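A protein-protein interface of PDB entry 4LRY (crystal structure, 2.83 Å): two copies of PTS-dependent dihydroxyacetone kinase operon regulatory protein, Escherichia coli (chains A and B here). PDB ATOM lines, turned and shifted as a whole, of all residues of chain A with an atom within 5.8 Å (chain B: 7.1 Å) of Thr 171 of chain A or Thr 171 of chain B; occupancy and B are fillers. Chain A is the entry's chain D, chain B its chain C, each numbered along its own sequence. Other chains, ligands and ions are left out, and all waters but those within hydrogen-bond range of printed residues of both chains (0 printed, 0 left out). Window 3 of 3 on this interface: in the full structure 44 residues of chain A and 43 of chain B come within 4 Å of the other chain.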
ATOM      1  N   ARG A  71       9.778  26.756 -20.993  1.00  0.00           N
ATOM      2  CA  ARG A  71      10.365  25.687 -20.243  1.00  0.00           C
ATOM      3  C   ARG A  71       9.809  24.548 -21.013  1.00  0.00           C
ATOM      4  O   ARG A  71       8.693  24.624 -21.497  1.00  0.00           O
ATOM      5  CB  ARG A  71       9.841  25.636 -18.799  1.00  0.00           C
ATOM      6  CG  ARG A  71      10.569  24.604 -17.981  1.00  0.00           C
ATOM      7  CD  ARG A  71      10.018  24.321 -16.610  1.00  0.00           C
ATOM      8  NE  ARG A  71      10.516  23.016 -16.124  1.00  0.00           N
ATOM      9  CZ  ARG A  71      10.210  22.480 -14.947  1.00  0.00           C
ATOM     10  NH1 ARG A  71       9.415  23.111 -14.095  1.00  0.00           N
ATOM     11  NH2 ARG A  71      10.680  21.292 -14.638  1.00  0.00           N
ATOM     12  N   LYS A 129       6.311  12.410  -6.366  1.00  0.00           N
ATOM     13  CA  LYS A 129       7.138  12.612  -7.551  1.00  0.00           C
ATOM     14  C   LYS A 129       7.813  11.341  -8.045  1.00  0.00           C
ATOM     15  O   LYS A 129       8.562  10.707  -7.321  1.00  0.00           O
ATOM     16  CB  LYS A 129       8.235  13.613  -7.240  1.00  0.00           C
ATOM     17  CG  LYS A 129       9.115  13.958  -8.420  1.00  0.00           C
ATOM     18  CD  LYS A 129      10.273  14.718  -7.932  1.00  0.00           C
ATOM     19  CE  LYS A 129      11.132  15.252  -9.057  1.00  0.00           C
ATOM     20  NZ  LYS A 129      11.243  16.748  -9.078  1.00  0.00           N
ATOM     21  N   CYS A 165       7.968  16.714 -16.988  1.00  0.00           N
ATOM     22  CA  CYS A 165       9.076  17.351 -17.652  1.00  0.00           C
ATOM     23  C   CYS A 165      10.203  16.333 -17.959  1.00  0.00           C
ATOM     24  O   CYS A 165      10.322  15.283 -17.273  1.00  0.00           O
ATOM     25  CB  CYS A 165       9.573  18.486 -16.777  1.00  0.00           C
ATOM     26  SG  CYS A 165      10.464  17.987 -15.289  1.00  0.00           S
ATOM     27  N   GLN A 169      15.672  17.896 -16.257  1.00  0.00           N
ATOM     28  CA  GLN A 169      15.294  19.231 -15.941  1.00  0.00           C
ATOM     29  C   GLN A 169      14.309  19.365 -14.794  1.00  0.00           C
ATOM     30  O   GLN A 169      13.750  20.441 -14.668  1.00  0.00           O
ATOM     31  CB  GLN A 169      14.708  19.882 -17.184  1.00  0.00           C
ATOM     32  CG  GLN A 169      15.612  19.837 -18.412  1.00  0.00           C
ATOM     33  CD  GLN A 169      14.946  20.353 -19.678  1.00  0.00           C
ATOM     34  OE1 GLN A 169      14.141  21.253 -19.641  1.00  0.00           O
ATOM     35  NE2 GLN A 169      15.297  19.787 -20.801  1.00  0.00           N
ATOM     36  N   THR A 170      14.066  18.338 -13.952  1.00  0.00           N
ATOM     37  CA  THR A 170      13.191  18.577 -12.776  1.00  0.00           C
ATOM     38  C   THR A 170      13.904  19.436 -11.825  1.00  0.00           C
ATOM     39  O   THR A 170      15.132  19.328 -11.682  1.00  0.00           O
ATOM     40  CB  THR A 170      12.815  17.379 -11.856  1.00  0.00           C
ATOM     41  OG1 THR A 170      13.620  16.241 -12.143  1.00  0.00           O
ATOM     42  CG2 THR A 170      11.318  17.055 -11.941  1.00  0.00           C
ATOM     43  N   THR A 171      13.098  20.239 -11.139  1.00  0.00           N
ATOM     44  CA  THR A 171      13.541  21.230 -10.156  1.00  0.00           C
ATOM     45  C   THR A 171      12.906  20.865  -8.832  1.00  0.00           C
ATOM     46  O   THR A 171      11.857  20.233  -8.804  1.00  0.00           O
ATOM     47  CB  THR A 171      13.038  22.651 -10.528  1.00  0.00           C
ATOM     48  OG1 THR A 171      11.630  22.761 -10.204  1.00  0.00           O
ATOM     49  CG2 THR A 171      13.262  22.941 -12.024  1.00  0.00           C
ATOM     50  N   ALA A 172      13.515  21.325  -7.746  1.00  0.00           N
ATOM     51  CA  ALA A 172      12.954  21.248  -6.399  1.00  0.00           C
ATOM     52  C   ALA A 172      11.570  21.910  -6.235  1.00  0.00           C
ATOM     53  O   ALA A 172      10.865  21.626  -5.269  1.00  0.00           O
ATOM     54  CB  ALA A 172      13.929  21.849  -5.415  1.00  0.00           C
ATOM     55  N   ALA A 173      11.178  22.783  -7.158  1.00  0.00           N
ATOM     56  CA  ALA A 173       9.961  23.548  -6.986  1.00  0.00           C
ATOM     57  C   ALA A 173       8.760  22.849  -7.588  1.00  0.00           C
ATOM     58  O   ALA A 173       7.603  23.214  -7.303  1.00  0.00           O
ATOM     59  CB  ALA A 173      10.127  24.930  -7.570  1.00  0.00           C
ATOM     60  N   ASP A 174       9.052  21.833  -8.399  1.00  0.00           N
ATOM     61  CA  ASP A 174       8.048  21.201  -9.218  1.00  0.00           C
ATOM     62  C   ASP A 174       6.923  20.516  -8.425  1.00  0.00           C
ATOM     63  O   ASP A 174       5.766  20.663  -8.754  1.00  0.00           O
ATOM     64  CB  ASP A 174       8.715  20.189 -10.148  1.00  0.00           C
ATOM     65  CG  ASP A 174       9.404  20.834 -11.351  1.00  0.00           C
ATOM     66  OD1 ASP A 174       9.092  22.000 -11.704  1.00  0.00           O
ATOM     67  OD2 ASP A 174      10.246  20.149 -11.974  1.00  0.00           O
ATOM     68  N   LEU A 175       7.248  19.735  -7.403  1.00  0.00           N
ATOM     69  CA  LEU A 175       6.220  19.066  -6.679  1.00  0.00           C
ATOM     70  C   LEU A 175       5.463  20.133  -5.942  1.00  0.00           C
ATOM     71  O   LEU A 175       4.268  20.305  -6.159  1.00  0.00           O
ATOM     72  CB  LEU A 175       6.801  18.055  -5.753  1.00  0.00           C
ATOM     73  CG  LEU A 175       5.810  17.154  -5.045  1.00  0.00           C
ATOM     74  CD1 LEU A 175       4.827  16.469  -5.984  1.00  0.00           C
ATOM     75  CD2 LEU A 175       6.585  16.132  -4.303  1.00  0.00           C
ATOM     76  N   MET B  68       9.375  20.430  -0.207  1.00  0.00           N
ATOM     77  CA  MET B  68      10.523  20.966  -0.898  1.00  0.00           C
ATOM     78  C   MET B  68      11.812  20.616  -0.140  1.00  0.00           C
ATOM     79  O   MET B  68      12.865  20.420  -0.768  1.00  0.00           O
ATOM     80  CB  MET B  68      10.369  22.464  -0.995  1.00  0.00           C
ATOM     81  CG  MET B  68      11.434  23.165  -1.761  1.00  0.00           C
ATOM     82  SD  MET B  68      10.762  24.758  -2.333  1.00  0.00           S
ATOM     83  CE  MET B  68      10.617  24.377  -4.030  1.00  0.00           C
ATOM     84  N   ARG B  71      16.564  21.864   0.682  1.00  0.00           N
ATOM     85  CA  ARG B  71      16.806  22.847  -0.351  1.00  0.00           C
ATOM     86  C   ARG B  71      17.104  24.082   0.427  1.00  0.00           C
ATOM     87  O   ARG B  71      16.603  24.245   1.560  1.00  0.00           O
ATOM     88  CB  ARG B  71      15.574  23.132  -1.218  1.00  0.00           C
ATOM     89  CG  ARG B  71      15.731  24.410  -2.000  1.00  0.00           C
ATOM     90  CD  ARG B  71      14.744  24.617  -3.114  1.00  0.00           C
ATOM     91  NE  ARG B  71      15.167  25.763  -3.934  1.00  0.00           N
ATOM     92  CZ  ARG B  71      14.375  26.444  -4.759  1.00  0.00           C
ATOM     93  NH1 ARG B  71      13.101  26.114  -4.853  1.00  0.00           N
ATOM     94  NH2 ARG B  71      14.850  27.455  -5.485  1.00  0.00           N
ATOM     95  N   LYS B 129      10.414  38.148 -11.021  1.00  0.00           N
ATOM     96  CA  LYS B 129      11.610  37.516 -10.522  1.00  0.00           C
ATOM     97  C   LYS B 129      12.753  38.466 -10.750  1.00  0.00           C
ATOM     98  O   LYS B 129      12.908  38.977 -11.874  1.00  0.00           O
ATOM     99  CB  LYS B 129      11.897  36.211 -11.255  1.00  0.00           C
ATOM    100  CG  LYS B 129      12.958  35.389 -10.585  1.00  0.00           C
ATOM    101  CD  LYS B 129      13.627  34.458 -11.550  1.00  0.00           C
ATOM    102  CE  LYS B 129      13.162  32.976 -11.390  1.00  0.00           C
ATOM    103  NZ  LYS B 129      14.308  32.028 -11.272  1.00  0.00           N
ATOM    104  N   ALA B 144      18.468  35.206  -5.835  1.00  0.00           N
ATOM    105  CA  ALA B 144      17.278  35.322  -6.630  1.00  0.00           C
ATOM    106  C   ALA B 144      16.134  35.473  -5.684  1.00  0.00           C
ATOM    107  O   ALA B 144      16.036  34.777  -4.678  1.00  0.00           O
ATOM    108  CB  ALA B 144      17.117  34.135  -7.413  1.00  0.00           C
ATOM    109  N   CYS B 146      11.928  35.650  -5.966  1.00  0.00           N
ATOM    110  CA  CYS B 146      10.661  35.751  -6.672  1.00  0.00           C
ATOM    111  C   CYS B 146       9.622  36.227  -5.679  1.00  0.00           C
ATOM    112  O   CYS B 146       9.653  35.821  -4.494  1.00  0.00           O
ATOM    113  CB  CYS B 146      10.214  34.405  -7.236  1.00  0.00           C
ATOM    114  SG  CYS B 146      11.517  33.411  -7.958  1.00  0.00           S
ATOM    115  N   CYS B 165      16.425  32.554  -2.745  1.00  0.00           N
ATOM    116  CA  CYS B 165      17.405  31.459  -2.798  1.00  0.00           C
ATOM    117  C   CYS B 165      18.678  31.967  -3.483  1.00  0.00           C
ATOM    118  O   CYS B 165      18.604  32.924  -4.293  1.00  0.00           O
ATOM    119  CB  CYS B 165      16.853  30.276  -3.577  1.00  0.00           C
ATOM    120  SG  CYS B 165      16.807  30.539  -5.363  1.00  0.00           S
ATOM    121  N   VAL B 167      21.302  32.780  -6.005  1.00  0.00           N
ATOM    122  CA  VAL B 167      21.053  32.854  -7.451  1.00  0.00           C
ATOM    123  C   VAL B 167      21.312  31.549  -8.269  1.00  0.00           C
ATOM    124  O   VAL B 167      20.546  31.248  -9.117  1.00  0.00           O
ATOM    125  CB  VAL B 167      21.802  34.031  -8.089  1.00  0.00           C
ATOM    126  CG1 VAL B 167      23.287  33.742  -8.147  1.00  0.00           C
ATOM    127  CG2 VAL B 167      21.251  34.321  -9.443  1.00  0.00           C
ATOM    128  N   GLU B 168      22.372  30.785  -8.008  1.00  0.00           N
ATOM    129  CA  GLU B 168      22.776  29.662  -8.899  1.00  0.00           C
ATOM    130  C   GLU B 168      21.756  28.599  -8.811  1.00  0.00           C
ATOM    131  O   GLU B 168      21.776  27.655  -9.582  1.00  0.00           O
ATOM    132  CB  GLU B 168      24.092  28.983  -8.499  1.00  0.00           C
ATOM    133  CG  GLU B 168      25.102  29.891  -7.814  1.00  0.00           C
ATOM    134  CD  GLU B 168      24.964  29.846  -6.299  1.00  0.00           C
ATOM    135  OE1 GLU B 168      24.792  28.679  -5.797  1.00  0.00           O
ATOM    136  OE2 GLU B 168      25.021  30.949  -5.642  1.00  0.00           O
ATOM    137  N   GLN B 169      20.878  28.718  -7.834  1.00  0.00           N
ATOM    138  CA  GLN B 169      19.926  27.691  -7.608  1.00  0.00           C
ATOM    139  C   GLN B 169      18.523  28.028  -8.070  1.00  0.00           C
ATOM    140  O   GLN B 169      17.631  27.249  -7.800  1.00  0.00           O
ATOM    141  CB  GLN B 169      19.959  27.289  -6.150  1.00  0.00           C
ATOM    142  CG  GLN B 169      21.280  26.640  -5.827  1.00  0.00           C
ATOM    143  CD  GLN B 169      21.356  25.991  -4.440  1.00  0.00           C
ATOM    144  OE1 GLN B 169      20.347  25.647  -3.828  1.00  0.00           O
ATOM    145  NE2 GLN B 169      22.569  25.845  -3.940  1.00  0.00           N
ATOM    146  N   THR B 170      18.279  29.136  -8.770  1.00  0.00           N
ATOM    147  CA  THR B 170      16.874  29.378  -9.076  1.00  0.00           C
ATOM    148  C   THR B 170      16.484  28.424 -10.139  1.00  0.00           C
ATOM    149  O   THR B 170      17.299  28.080 -10.966  1.00  0.00           O
ATOM    150  CB  THR B 170      16.491  30.748  -9.650  1.00  0.00           C
ATOM    151  OG1 THR B 170      17.554  31.279 -10.441  1.00  0.00           O
ATOM    152  CG2 THR B 170      16.066  31.668  -8.584  1.00  0.00           C
ATOM    153  N   THR B 171      15.217  28.056 -10.140  1.00  0.00           N
ATOM    154  CA  THR B 171      14.673  27.064 -11.042  1.00  0.00           C
ATOM    155  C   THR B 171      13.530  27.768 -11.786  1.00  0.00           C
ATOM    156  O   THR B 171      13.142  28.874 -11.409  1.00  0.00           O
ATOM    157  CB  THR B 171      14.126  25.863 -10.221  1.00  0.00           C
ATOM    158  OG1 THR B 171      12.883  26.224  -9.573  1.00  0.00           O
ATOM    159  CG2 THR B 171      15.144  25.412  -9.125  1.00  0.00           C
ATOM    160  N   ALA B 172      12.965  27.149 -12.823  1.00  0.00           N
ATOM    161  CA  ALA B 172      11.897  27.835 -13.529  1.00  0.00           C
ATOM    162  C   ALA B 172      10.568  27.726 -12.818  1.00  0.00           C
ATOM    163  O   ALA B 172       9.692  28.505 -13.106  1.00  0.00           O
ATOM    164  CB  ALA B 172      11.787  27.387 -14.913  1.00  0.00           C
ATOM    165  N   ALA B 173      10.409  26.774 -11.897  1.00  0.00           N
ATOM    166  CA  ALA B 173       9.187  26.676 -11.098  1.00  0.00           C
ATOM    167  C   ALA B 173       9.116  27.734  -9.969  1.00  0.00           C
ATOM    168  O   ALA B 173       8.014  28.114  -9.568  1.00  0.00           O
ATOM    169  CB  ALA B 173       9.004  25.293 -10.550  1.00  0.00           C
ATOM    170  N   ASP B 174      10.247  28.237  -9.475  1.00  0.00           N
ATOM    171  CA  ASP B 174      10.204  29.238  -8.393  1.00  0.00           C
ATOM    172  C   ASP B 174       9.167  30.390  -8.552  1.00  0.00           C
ATOM    173  O   ASP B 174       8.297  30.552  -7.693  1.00  0.00           O
ATOM    174  CB  ASP B 174      11.581  29.793  -8.104  1.00  0.00           C
ATOM    175  CG  ASP B 174      12.556  28.727  -7.645  1.00  0.00           C
ATOM    176  OD1 ASP B 174      12.134  27.748  -7.012  1.00  0.00           O
ATOM    177  OD2 ASP B 174      13.769  28.872  -7.910  1.00  0.00           O
ATOM    178  N   LEU B 175       9.226  31.166  -9.630  1.00  0.00           N
ATOM    179  CA  LEU B 175       8.213  32.187  -9.848  1.00  0.00           C
ATOM    180  C   LEU B 175       6.795  31.625  -9.756  1.00  0.00           C
ATOM    181  O   LEU B 175       6.050  32.031  -8.875  1.00  0.00           O
ATOM    182  CB  LEU B 175       8.422  32.981 -11.149  1.00  0.00           C
ATOM    183  CG  LEU B 175       7.642  34.306 -11.150  1.00  0.00           C
ATOM    184  CD1 LEU B 175       7.889  35.043  -9.871  1.00  0.00           C
ATOM    185  CD2 LEU B 175       7.921  35.197 -12.345  1.00  0.00           C
ATOM    186  N   PRO B 176       6.415  30.657 -10.627  1.00  0.00           N
ATOM    187  CA  PRO B 176       5.032  30.149 -10.573  1.00  0.00           C
ATOM    188  C   PRO B 176       4.649  29.532  -9.227  1.00  0.00           C
ATOM    189  O   PRO B 176       3.462  29.531  -8.880  1.00  0.00           O
ATOM    190  CB  PRO B 176       5.000  29.056 -11.648  1.00  0.00           C
ATOM    191  CG  PRO B 176       6.097  29.311 -12.511  1.00  0.00           C
ATOM    192  CD  PRO B 176       7.183  29.940 -11.656  1.00  0.00           C
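The side-chain sulfur (SG) of Cys 165 of chain A is in hydrogen-bond range of the guanidinium group (NH2) of Arg 71 of chain A.
The side-chain sulfur (SD) of Met 68 of chain B lies close to the guanidinium group (NH1) of Arg 71 of chain B.
The guanidinium group (NH2) of Arg 71 of chain B lies within hydrogen-bond range of the side-chain sulfur (SG) of Cys 165 of chain B (3.7 Å).
The side-chain carboxylate of Asp 174 of chain B lies within hydrogen-bond range of the backbone NH of Thr 171 of chain B (2.8 Å).
NZ of Lys 129 of chain B is in hydrogen-bond range of O of Thr 171 of chain B.
The side-chain hydroxyl (OG1) of Thr 171 of chain A lies close to the backbone NH (N) of Ala 173 of chain A.
Among the printed residues, pairs that only touch across the chains: Arg 71 of chain A with Ala 172 of chain B (3.9 Å), Thr 171 of chain A with Thr 171 of chain B (3.4 Å), Thr 171 of chain A with Ala 173 of chain B (3.7 Å), Ala 172 of chain A with Met 68 of chain B (3.0 Å), Ala 172 of chain A with Arg 71 of chain B (3.7 Å), Ala 173 of chain A with Met 68 of chain B (3.1 Å), Ala 173 of chain A with Thr 171 of chain B (3.6 Å), Ala 173 of chain A with Ala 173 of chain B (3.2 Å), Ala 173 of chain A with Asp 174 of chain B (3.5 Å) and Asp 174 of chain A with Ala 173 of chain B (3.5 Å).
Thr 171 of chain A touches just these residues of chain B: Thr 171 and Ala 173.
Printed residues of chain A within 4 Å of Arg 71 of chain B: Ala 172 (3.7 Å).
Lys 129 of chain B touches none of the printed residues of chain A.
Thr 171 of chain B touches just these residues of chain A: Thr 171 and Ala 173.
Of the printed residues of chain A, Ala 172 of chain B touches Arg 71.
Of the printed residues of chain A, Asp 174 of chain B touches Ala 173.
The nearest residue of chain B that does not touch Thr 171 of chain A is Ala 172 of chain B (4.3 Å).
The nearest printed residue of chain A that does not touch Ala 172 of chain B is Thr 171 of chain A (4.3 Å).
Along chain B the printed residues that touch a printed residue of chain A span positions 68 to 174.
Among the printed residues, no Asp or Glu carboxylate lies within 4 Å of a Lys or Arg side-chain nitrogen of the other chain.
Arg 71 of chain A touches Ala 172 of chain B, and with the chains exchanged Ala 172 of chain A touches Arg 71 of chain B.
Thr 171 of chain A touches its own counterpart, Thr 171 of chain B.
Thr 171 of chain A touches Ala 173 of chain B, and with the chains exchanged Ala 173 of chain A touches Thr 171 of chain B.
Ala 173 of chain A touches Asp 174 of chain B, and with the chains exchanged Asp 174 of chain A touches Ala 173 of chain B.
Positions printed for both chains: 71, 129, 165, 169, 170, 171, 172, 173, 174 and 175.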
